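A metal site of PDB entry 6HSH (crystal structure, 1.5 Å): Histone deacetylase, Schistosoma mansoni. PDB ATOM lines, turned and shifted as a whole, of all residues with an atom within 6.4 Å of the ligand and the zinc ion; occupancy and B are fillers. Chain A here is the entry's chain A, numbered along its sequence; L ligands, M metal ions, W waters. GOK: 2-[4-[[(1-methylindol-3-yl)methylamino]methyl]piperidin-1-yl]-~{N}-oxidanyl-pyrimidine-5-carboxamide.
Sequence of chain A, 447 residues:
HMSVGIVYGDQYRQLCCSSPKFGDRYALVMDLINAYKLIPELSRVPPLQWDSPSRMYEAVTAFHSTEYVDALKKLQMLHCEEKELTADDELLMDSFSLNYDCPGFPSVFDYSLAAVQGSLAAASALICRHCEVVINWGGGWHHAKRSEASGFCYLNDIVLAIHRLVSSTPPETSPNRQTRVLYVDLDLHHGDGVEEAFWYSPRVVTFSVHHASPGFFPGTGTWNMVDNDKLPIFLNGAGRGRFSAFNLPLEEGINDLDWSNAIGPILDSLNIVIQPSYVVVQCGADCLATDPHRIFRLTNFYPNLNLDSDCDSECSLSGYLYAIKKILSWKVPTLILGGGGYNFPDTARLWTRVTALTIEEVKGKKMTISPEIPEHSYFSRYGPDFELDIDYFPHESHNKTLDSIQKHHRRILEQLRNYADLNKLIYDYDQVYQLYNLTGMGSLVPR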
ATOM      1  N   PHE A  22      11.450  25.858 -12.429  1.00  0.00           N
ATOM      2  CA  PHE A  22      12.667  25.855 -13.224  1.00  0.00           C
ATOM      3  C   PHE A  22      12.533  26.683 -14.499  1.00  0.00           C
ATOM      4  O   PHE A  22      13.507  26.786 -15.241  1.00  0.00           O
ATOM      5  CB  PHE A  22      13.096  24.423 -13.560  1.00  0.00           C
ATOM      6  CG  PHE A  22      13.617  23.670 -12.359  1.00  0.00           C
ATOM      7  CD1 PHE A  22      14.865  23.973 -11.837  1.00  0.00           C
ATOM      8  CD2 PHE A  22      12.846  22.706 -11.736  1.00  0.00           C
ATOM      9  CE1 PHE A  22      15.334  23.312 -10.723  1.00  0.00           C
ATOM     10  CE2 PHE A  22      13.315  22.044 -10.622  1.00  0.00           C
ATOM     11  CZ  PHE A  22      14.563  22.345 -10.110  1.00  0.00           C
ATOM     12  N   TYR A 100       2.353  22.079  -1.577  1.00  0.00           N
ATOM     13  CA  TYR A 100       3.385  23.004  -1.125  1.00  0.00           C
ATOM     14  C   TYR A 100       4.581  23.031  -2.066  1.00  0.00           C
ATOM     15  O   TYR A 100       4.639  23.827  -3.008  1.00  0.00           O
ATOM     16  CB  TYR A 100       3.853  22.641   0.299  1.00  0.00           C
ATOM     17  CG  TYR A 100       2.750  22.480   1.333  1.00  0.00           C
ATOM     18  CD1 TYR A 100       1.992  23.572   1.752  1.00  0.00           C
ATOM     19  CD2 TYR A 100       2.496  21.241   1.912  1.00  0.00           C
ATOM     20  CE1 TYR A 100       0.985  23.425   2.717  1.00  0.00           C
ATOM     21  CE2 TYR A 100       1.482  21.086   2.870  1.00  0.00           C
ATOM     22  CZ  TYR A 100       0.730  22.181   3.267  1.00  0.00           C
ATOM     23  OH  TYR A 100      -0.257  22.037   4.210  1.00  0.00           O
ATOM     24  N   ASP A 101       5.545  22.156  -1.802  1.00  0.00           N
ATOM     25  CA  ASP A 101       6.799  22.141  -2.545  1.00  0.00           C
ATOM     26  C   ASP A 101       6.680  21.462  -3.897  1.00  0.00           C
ATOM     27  O   ASP A 101       7.531  21.695  -4.759  1.00  0.00           O
ATOM     28  CB  ASP A 101       7.857  21.442  -1.698  1.00  0.00           C
ATOM     29  CG  ASP A 101       7.933  22.040  -0.319  1.00  0.00           C
ATOM     30  OD1 ASP A 101       8.251  23.250  -0.263  1.00  0.00           O
ATOM     31  OD2 ASP A 101       7.645  21.335   0.668  1.00  0.00           O
ATOM     32  N   HIS A 142      16.082  13.325  -8.391  1.00  0.00           N
ATOM     33  CA  HIS A 142      16.496  12.222  -7.515  1.00  0.00           C
ATOM     34  C   HIS A 142      15.645  12.074  -6.250  1.00  0.00           C
ATOM     35  O   HIS A 142      15.796  11.052  -5.571  1.00  0.00           O
ATOM     36  CB  HIS A 142      17.983  12.375  -7.119  1.00  0.00           C
ATOM     37  CG  HIS A 142      18.351  13.690  -6.484  1.00  0.00           C
ATOM     38  ND1 HIS A 142      19.598  13.909  -5.946  1.00  0.00           N
ATOM     39  CD2 HIS A 142      17.667  14.845  -6.326  1.00  0.00           C
ATOM     40  CE1 HIS A 142      19.667  15.145  -5.475  1.00  0.00           C
ATOM     41  NE2 HIS A 142      18.508  15.735  -5.694  1.00  0.00           N
ATOM     42  N   HIS A 143      14.752  13.019  -5.930  1.00  0.00           N
ATOM     43  CA  HIS A 143      14.001  12.968  -4.679  1.00  0.00           C
ATOM     44  C   HIS A 143      12.679  12.218  -4.764  1.00  0.00           C
ATOM     45  O   HIS A 143      12.131  11.830  -3.713  1.00  0.00           O
ATOM     46  CB  HIS A 143      13.699  14.393  -4.185  1.00  0.00           C
ATOM     47  CG  HIS A 143      14.910  15.166  -3.763  1.00  0.00           C
ATOM     48  ND1 HIS A 143      15.859  14.644  -2.904  1.00  0.00           N
ATOM     49  CD2 HIS A 143      15.292  16.436  -4.027  1.00  0.00           C
ATOM     50  CE1 HIS A 143      16.787  15.561  -2.689  1.00  0.00           C
ATOM     51  NE2 HIS A 143      16.468  16.660  -3.354  1.00  0.00           N
ATOM     52  N   SER A 150       8.549  14.916  -4.029  1.00  0.00           N
ATOM     53  CA  SER A 150       9.408  15.474  -2.997  1.00  0.00           C
ATOM     54  C   SER A 150      10.432  16.408  -3.616  1.00  0.00           C
ATOM     55  O   SER A 150      11.001  16.098  -4.656  1.00  0.00           O
ATOM     56  CB  SER A 150      10.141  14.355  -2.256  1.00  0.00           C
ATOM     57  OG  SER A 150      11.018  14.920  -1.298  1.00  0.00           O
ATOM     58  N   GLY A 151      10.706  17.523  -2.938  1.00  0.00           N
ATOM     59  CA  GLY A 151      11.837  18.336  -3.356  1.00  0.00           C
ATOM     60  C   GLY A 151      11.788  18.812  -4.802  1.00  0.00           C
ATOM     61  O   GLY A 151      12.826  18.836  -5.470  1.00  0.00           O
ATOM     62  N   PHE A 152      10.620  19.218  -5.271  1.00  0.00           N
ATOM     63  CA  PHE A 152      10.375  19.652  -6.648  1.00  0.00           C
ATOM     64  C   PHE A 152      10.468  18.510  -7.665  1.00  0.00           C
ATOM     65  O   PHE A 152      10.503  18.780  -8.872  1.00  0.00           O
ATOM     66  CB  PHE A 152      11.333  20.783  -7.108  1.00  0.00           C
ATOM     67  CG  PHE A 152      11.701  21.782  -6.024  1.00  0.00           C
ATOM     68  CD1 PHE A 152      10.731  22.317  -5.182  1.00  0.00           C
ATOM     69  CD2 PHE A 152      13.020  22.212  -5.878  1.00  0.00           C
ATOM     70  CE1 PHE A 152      11.072  23.232  -4.193  1.00  0.00           C
ATOM     71  CE2 PHE A 152      13.360  23.141  -4.892  1.00  0.00           C
ATOM     72  CZ  PHE A 152      12.376  23.647  -4.053  1.00  0.00           C
ATOM     73  N   CYS A 153      10.504  17.256  -7.221  1.00  0.00           N
ATOM     74  CA  CYS A 153      10.624  16.092  -8.093  1.00  0.00           C
ATOM     75  C   CYS A 153       9.321  15.321  -8.062  1.00  0.00           C
ATOM     76  O   CYS A 153       8.833  14.997  -6.976  1.00  0.00           O
ATOM     77  CB  CYS A 153      11.758  15.157  -7.642  1.00  0.00           C
ATOM     78  SG  CYS A 153      13.389  15.907  -7.613  1.00  0.00           S
ATOM     79  N   ASP A 187      24.767  16.380  -6.590  1.00  0.00           N
ATOM     80  CA  ASP A 187      23.889  17.467  -6.165  1.00  0.00           C
ATOM     81  C   ASP A 187      24.240  17.973  -4.761  1.00  0.00           C
ATOM     82  O   ASP A 187      24.773  17.236  -3.921  1.00  0.00           O
ATOM     83  CB  ASP A 187      22.434  16.967  -6.159  1.00  0.00           C
ATOM     84  CG  ASP A 187      21.415  18.073  -6.200  1.00  0.00           C
ATOM     85  OD1 ASP A 187      21.057  18.581  -5.128  1.00  0.00           O
ATOM     86  OD2 ASP A 187      20.911  18.392  -7.297  1.00  0.00           O
ATOM     87  N   LEU A 188      23.890  19.235  -4.478  1.00  0.00           N
ATOM     88  CA  LEU A 188      24.019  19.755  -3.126  1.00  0.00           C
ATOM     89  C   LEU A 188      23.234  18.917  -2.109  1.00  0.00           C
ATOM     90  O   LEU A 188      23.639  18.807  -0.946  1.00  0.00           O
ATOM     91  CB  LEU A 188      23.564  21.207  -3.058  1.00  0.00           C
ATOM     92  CG  LEU A 188      23.669  21.890  -1.686  1.00  0.00           C
ATOM     93  CD1 LEU A 188      25.122  22.066  -1.283  1.00  0.00           C
ATOM     94  CD2 LEU A 188      22.958  23.241  -1.749  1.00  0.00           C
ATOM     95  N   HIS A 189      22.126  18.330  -2.532  1.00  0.00           N
ATOM     96  CA  HIS A 189      21.276  17.614  -1.597  1.00  0.00           C
ATOM     97  C   HIS A 189      21.466  16.103  -1.722  1.00  0.00           C
ATOM     98  O   HIS A 189      21.882  15.561  -2.749  1.00  0.00           O
ATOM     99  CB  HIS A 189      19.809  17.986  -1.809  1.00  0.00           C
ATOM    100  CG  HIS A 189      19.568  19.455  -1.715  1.00  0.00           C
ATOM    101  ND1 HIS A 189      19.720  20.296  -2.792  1.00  0.00           N
ATOM    102  CD2 HIS A 189      19.257  20.247  -0.659  1.00  0.00           C
ATOM    103  CE1 HIS A 189      19.451  21.537  -2.427  1.00  0.00           C
ATOM    104  NE2 HIS A 189      19.185  21.533  -1.128  1.00  0.00           N
ATOM    105  N   HIS A 190      21.127  15.420  -0.624  1.00  0.00           N
ATOM    106  CA  HIS A 190      21.211  13.956  -0.590  1.00  0.00           C
ATOM    107  C   HIS A 190      20.259  13.324  -1.603  1.00  0.00           C
ATOM    108  O   HIS A 190      19.075  13.661  -1.650  1.00  0.00           O
ATOM    109  CB  HIS A 190      20.891  13.478   0.824  1.00  0.00           C
ATOM    110  CG  HIS A 190      20.837  11.990   0.951  1.00  0.00           C
ATOM    111  ND1 HIS A 190      19.742  11.309   1.454  1.00  0.00           N
ATOM    112  CD2 HIS A 190      21.736  11.033   0.602  1.00  0.00           C
ATOM    113  CE1 HIS A 190      19.990  10.013   1.437  1.00  0.00           C
ATOM    114  NE2 HIS A 190      21.195   9.815   0.936  1.00  0.00           N
ATOM    115  N   PHE A 217      17.201  20.209   3.917  1.00  0.00           N
ATOM    116  CA  PHE A 217      16.540  19.184   3.088  1.00  0.00           C
ATOM    117  C   PHE A 217      17.502  18.153   2.475  1.00  0.00           C
ATOM    118  O   PHE A 217      18.573  18.537   2.031  1.00  0.00           O
ATOM    119  CB  PHE A 217      15.767  19.885   1.971  1.00  0.00           C
ATOM    120  CG  PHE A 217      14.876  18.966   1.194  1.00  0.00           C
ATOM    121  CD1 PHE A 217      13.618  18.659   1.684  1.00  0.00           C
ATOM    122  CD2 PHE A 217      15.299  18.419  -0.006  1.00  0.00           C
ATOM    123  CE1 PHE A 217      12.789  17.812   0.981  1.00  0.00           C
ATOM    124  CE2 PHE A 217      14.476  17.563  -0.717  1.00  0.00           C
ATOM    125  CZ  PHE A 217      13.219  17.257  -0.218  1.00  0.00           C
ATOM    126  N   GLN A 282      24.467  12.097 -11.345  1.00  0.00           N
ATOM    127  CA  GLN A 282      23.563  13.232 -11.193  1.00  0.00           C
ATOM    128  C   GLN A 282      24.443  14.447 -10.932  1.00  0.00           C
ATOM    129  O   GLN A 282      25.311  14.415 -10.041  1.00  0.00           O
ATOM    130  CB  GLN A 282      22.563  12.991 -10.046  1.00  0.00           C
ATOM    131  CG  GLN A 282      21.292  13.868 -10.061  1.00  0.00           C
ATOM    132  CD  GLN A 282      21.482  15.181  -9.294  1.00  0.00           C
ATOM    133  OE1 GLN A 282      22.621  15.593  -9.033  1.00  0.00           O
ATOM    134  NE2 GLN A 282      20.366  15.830  -8.915  1.00  0.00           N
ATOM    135  N   GLY A 284      23.555  17.869 -10.387  1.00  0.00           N
ATOM    136  CA  GLY A 284      22.859  19.046  -9.896  1.00  0.00           C
ATOM    137  C   GLY A 284      23.828  20.179  -9.644  1.00  0.00           C
ATOM    138  O   GLY A 284      24.891  19.968  -9.065  1.00  0.00           O
ATOM    139  N   ASP A 286      23.586  22.965  -7.846  1.00  0.00           N
ATOM    140  CA  ASP A 286      23.381  23.831  -6.698  1.00  0.00           C
ATOM    141  C   ASP A 286      24.545  23.835  -5.716  1.00  0.00           C
ATOM    142  O   ASP A 286      24.464  24.524  -4.693  1.00  0.00           O
ATOM    143  CB  ASP A 286      22.062  23.497  -5.976  1.00  0.00           C
ATOM    144  CG  ASP A 286      21.735  22.008  -5.947  1.00  0.00           C
ATOM    145  OD1 ASP A 286      22.580  21.157  -6.273  1.00  0.00           O
ATOM    146  OD2 ASP A 286      20.586  21.723  -5.559  1.00  0.00           O
ATOM    147  N   HIS A 293      21.324  29.112  -2.997  1.00  0.00           N
ATOM    148  CA  HIS A 293      21.592  28.384  -1.758  1.00  0.00           C
ATOM    149  C   HIS A 293      22.845  28.912  -1.076  1.00  0.00           C
ATOM    150  O   HIS A 293      22.863  29.120   0.147  1.00  0.00           O
ATOM    151  CB  HIS A 293      21.755  26.884  -2.016  1.00  0.00           C
ATOM    152  CG  HIS A 293      20.465  26.141  -2.175  1.00  0.00           C
ATOM    153  ND1 HIS A 293      19.859  25.960  -3.405  1.00  0.00           N
ATOM    154  CD2 HIS A 293      19.679  25.512  -1.270  1.00  0.00           C
ATOM    155  CE1 HIS A 293      18.748  25.271  -3.237  1.00  0.00           C
ATOM    156  NE2 HIS A 293      18.609  24.980  -1.960  1.00  0.00           N
ATOM    157  N   GLY A 339      19.654  18.063 -12.636  1.00  0.00           N
ATOM    158  CA  GLY A 339      19.186  18.097 -11.263  1.00  0.00           C
ATOM    159  C   GLY A 339      18.976  19.509 -10.792  1.00  0.00           C
ATOM    160  O   GLY A 339      18.547  20.370 -11.579  1.00  0.00           O
ATOM    161  N   GLY A 340      19.280  19.779  -9.533  1.00  0.00           N
ATOM    162  CA  GLY A 340      19.184  21.133  -8.985  1.00  0.00           C
ATOM    163  C   GLY A 340      20.048  22.128  -9.740  1.00  0.00           C
ATOM    164  O   GLY A 340      20.881  21.810 -10.587  1.00  0.00           O
ATOM    165  N   GLY A 341      19.814  23.397  -9.413  1.00  0.00           N
ATOM    166  CA  GLY A 341      20.523  24.501 -10.029  1.00  0.00           C
ATOM    167  C   GLY A 341      19.583  25.663 -10.228  1.00  0.00           C
ATOM    168  O   GLY A 341      18.789  25.676 -11.170  1.00  0.00           O
ATOM    169  N   TYR A 342      19.644  26.643  -9.329  1.00  0.00           N
ATOM    170  CA  TYR A 342      18.650  27.691  -9.258  1.00  0.00           C
ATOM    171  C   TYR A 342      19.180  29.033  -9.738  1.00  0.00           C
ATOM    172  O   TYR A 342      18.418  30.008  -9.807  1.00  0.00           O
ATOM    173  CB  TYR A 342      18.101  27.739  -7.822  1.00  0.00           C
ATOM    174  CG  TYR A 342      17.649  26.329  -7.466  1.00  0.00           C
ATOM    175  CD1 TYR A 342      16.383  25.877  -7.835  1.00  0.00           C
ATOM    176  CD2 TYR A 342      18.522  25.429  -6.856  1.00  0.00           C
ATOM    177  CE1 TYR A 342      15.986  24.564  -7.572  1.00  0.00           C
ATOM    178  CE2 TYR A 342      18.132  24.125  -6.584  1.00  0.00           C
ATOM    179  CZ  TYR A 342      16.868  23.704  -6.939  1.00  0.00           C
ATOM    180  OH  TYR A 342      16.493  22.415  -6.661  1.00  0.00           O
HETATM  181  N1  GOK L   1      17.010  19.128  -4.226  1.00  0.00           N
HETATM  182  O3  GOK L   1      17.605  21.204  -4.851  1.00  0.00           O
HETATM  183  C5  GOK L   1      14.170  21.793  -1.286  1.00  0.00           C
HETATM  184  C8  GOK L   1      15.855  20.995  -3.255  1.00  0.00           C
HETATM  185  C9  GOK L   1      16.099  22.087  -2.438  1.00  0.00           C
HETATM  186  C14 GOK L   1      13.905  22.960   0.888  1.00  0.00           C
HETATM  187  N15 GOK L   1      13.455  22.028  -0.153  1.00  0.00           N
HETATM  188  C16 GOK L   1      12.175  21.377   0.159  1.00  0.00           C
HETATM  189  C34 GOK L   1       7.553  27.959   0.758  1.00  0.00           C
HETATM  190  C2  GOK L   1      16.883  20.460  -4.202  1.00  0.00           C
HETATM  191  O4  GOK L   1      18.057  18.497  -4.890  1.00  0.00           O
HETATM  192  N6  GOK L   1      13.774  20.757  -2.044  1.00  0.00           N
HETATM  193  C7  GOK L   1      14.629  20.388  -3.005  1.00  0.00           C
HETATM  194  N10 GOK L   1      15.289  22.504  -1.448  1.00  0.00           N
HETATM  195  C13 GOK L   1      12.843  24.015   1.176  1.00  0.00           C
HETATM  196  C17 GOK L   1      11.091  22.413   0.461  1.00  0.00           C
HETATM  197  C18 GOK L   1      11.509  23.392   1.556  1.00  0.00           C
HETATM  198  C27 GOK L   1      10.464  24.476   1.735  1.00  0.00           C
HETATM  199  N29 GOK L   1       9.128  23.951   2.026  1.00  0.00           N
HETATM  200  C30 GOK L   1       8.252  24.870   2.738  1.00  0.00           C
HETATM  201  C31 GOK L   1       8.167  26.233   2.112  1.00  0.00           C
HETATM  202  N32 GOK L   1       8.550  28.387   1.615  1.00  0.00           N
HETATM  203  C33 GOK L   1       8.898  27.337   2.423  1.00  0.00           C
HETATM  204  C35 GOK L   1       7.290  26.613   1.042  1.00  0.00           C
HETATM  205  C36 GOK L   1       6.294  25.964   0.310  1.00  0.00           C
HETATM  206  C37 GOK L   1       5.612  26.643  -0.685  1.00  0.00           C
HETATM  207  C38 GOK L   1       5.896  27.970  -0.956  1.00  0.00           C
HETATM  208  C39 GOK L   1       6.877  28.645  -0.238  1.00  0.00           C
HETATM  209  C44 GOK L   1       9.138  29.718   1.644  1.00  0.00           C
HETATM  210 ZN    ZN M   1      19.613  20.014  -4.996  1.00  0.00          ZN
HETATM  211  O   HOH W   1       9.377  22.128   4.120  1.00  0.00           O
HETATM  212  O   HOH W   2      17.280  17.847  -7.806  1.00  0.00           O
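An oxygen (O3) of the ligand lies close to the side-chain hydroxyl (OH) of Tyr 342 (2.4 Å). A nitrogen (N29) of the ligand lies within salt-bridge range of the side-chain carboxylate (OD1) of Asp 101 (2.5 Å). A ring nitrogen (NE2) of His 143 is in hydrogen-bond range of a nitrogen (N1) of the ligand, at 2.7 Å. An oxygen (O4) of the ligand lies close to a ring nitrogen (NE2) of His 142.
OD2 of Asp 187 lies within hydrogen-bond range of N of Gly 340, 3.1 Å away. The side-chain carboxylate (OD2) of Asp 187 lies within hydrogen-bond range of the side-chain amide nitrogen (NE2) of Gln 282 (3.1 Å). The side-chain carboxylate (OD1) of Asp 286 sits at hydrogen-bond distance from the backbone NH (N) of Leu 188, at 2.9 Å. A ring nitrogen (NE2) of His 142 is in hydrogen-bond range of a ring nitrogen (NE2) of His 143 (3.2 Å). SG of Cys 153 is in hydrogen-bond range of N of His 143 (3.6 Å). The backbone carbonyl oxygen (O) of Gly 151 sits at hydrogen-bond distance from the side-chain sulfur (SG) of Cys 153 (3.7 Å).
Merely in contact with the ligand: Gly 151, Phe 217, Phe 152, Tyr 100 and His 293. Hydrophobic or aromatic side chains that line the ligand: His 142, His 143, Phe 152, His 189, Phe 217 and Tyr 342. Within 4 Å of the ligand: Tyr 100, Asp 101, His 142, His 143, Gly 151, Phe 152, Asp 187, His 189, Phe 217, Asp 286, His 293 and Tyr 342.
Of the 22 residues printed, 3 come within 4 Å of the zinc ion. The nearest printed residue that does not touch the zinc ion is Gly 340 (4.2 Å).
The zinc ion is bound by OD1 of Asp 187 (2.0 Å), OD2 of Asp 286 (2.0 Å), O4 of the ligand (2.2 Å), ND1 of His 189 (2.2 Å) and O3 of the ligand (2.3 Å).
Water W2 bridges a ring nitrogen (NE2) of His 142 (3.2 Å) and the backbone NH of Gly 340 (3.3 Å).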
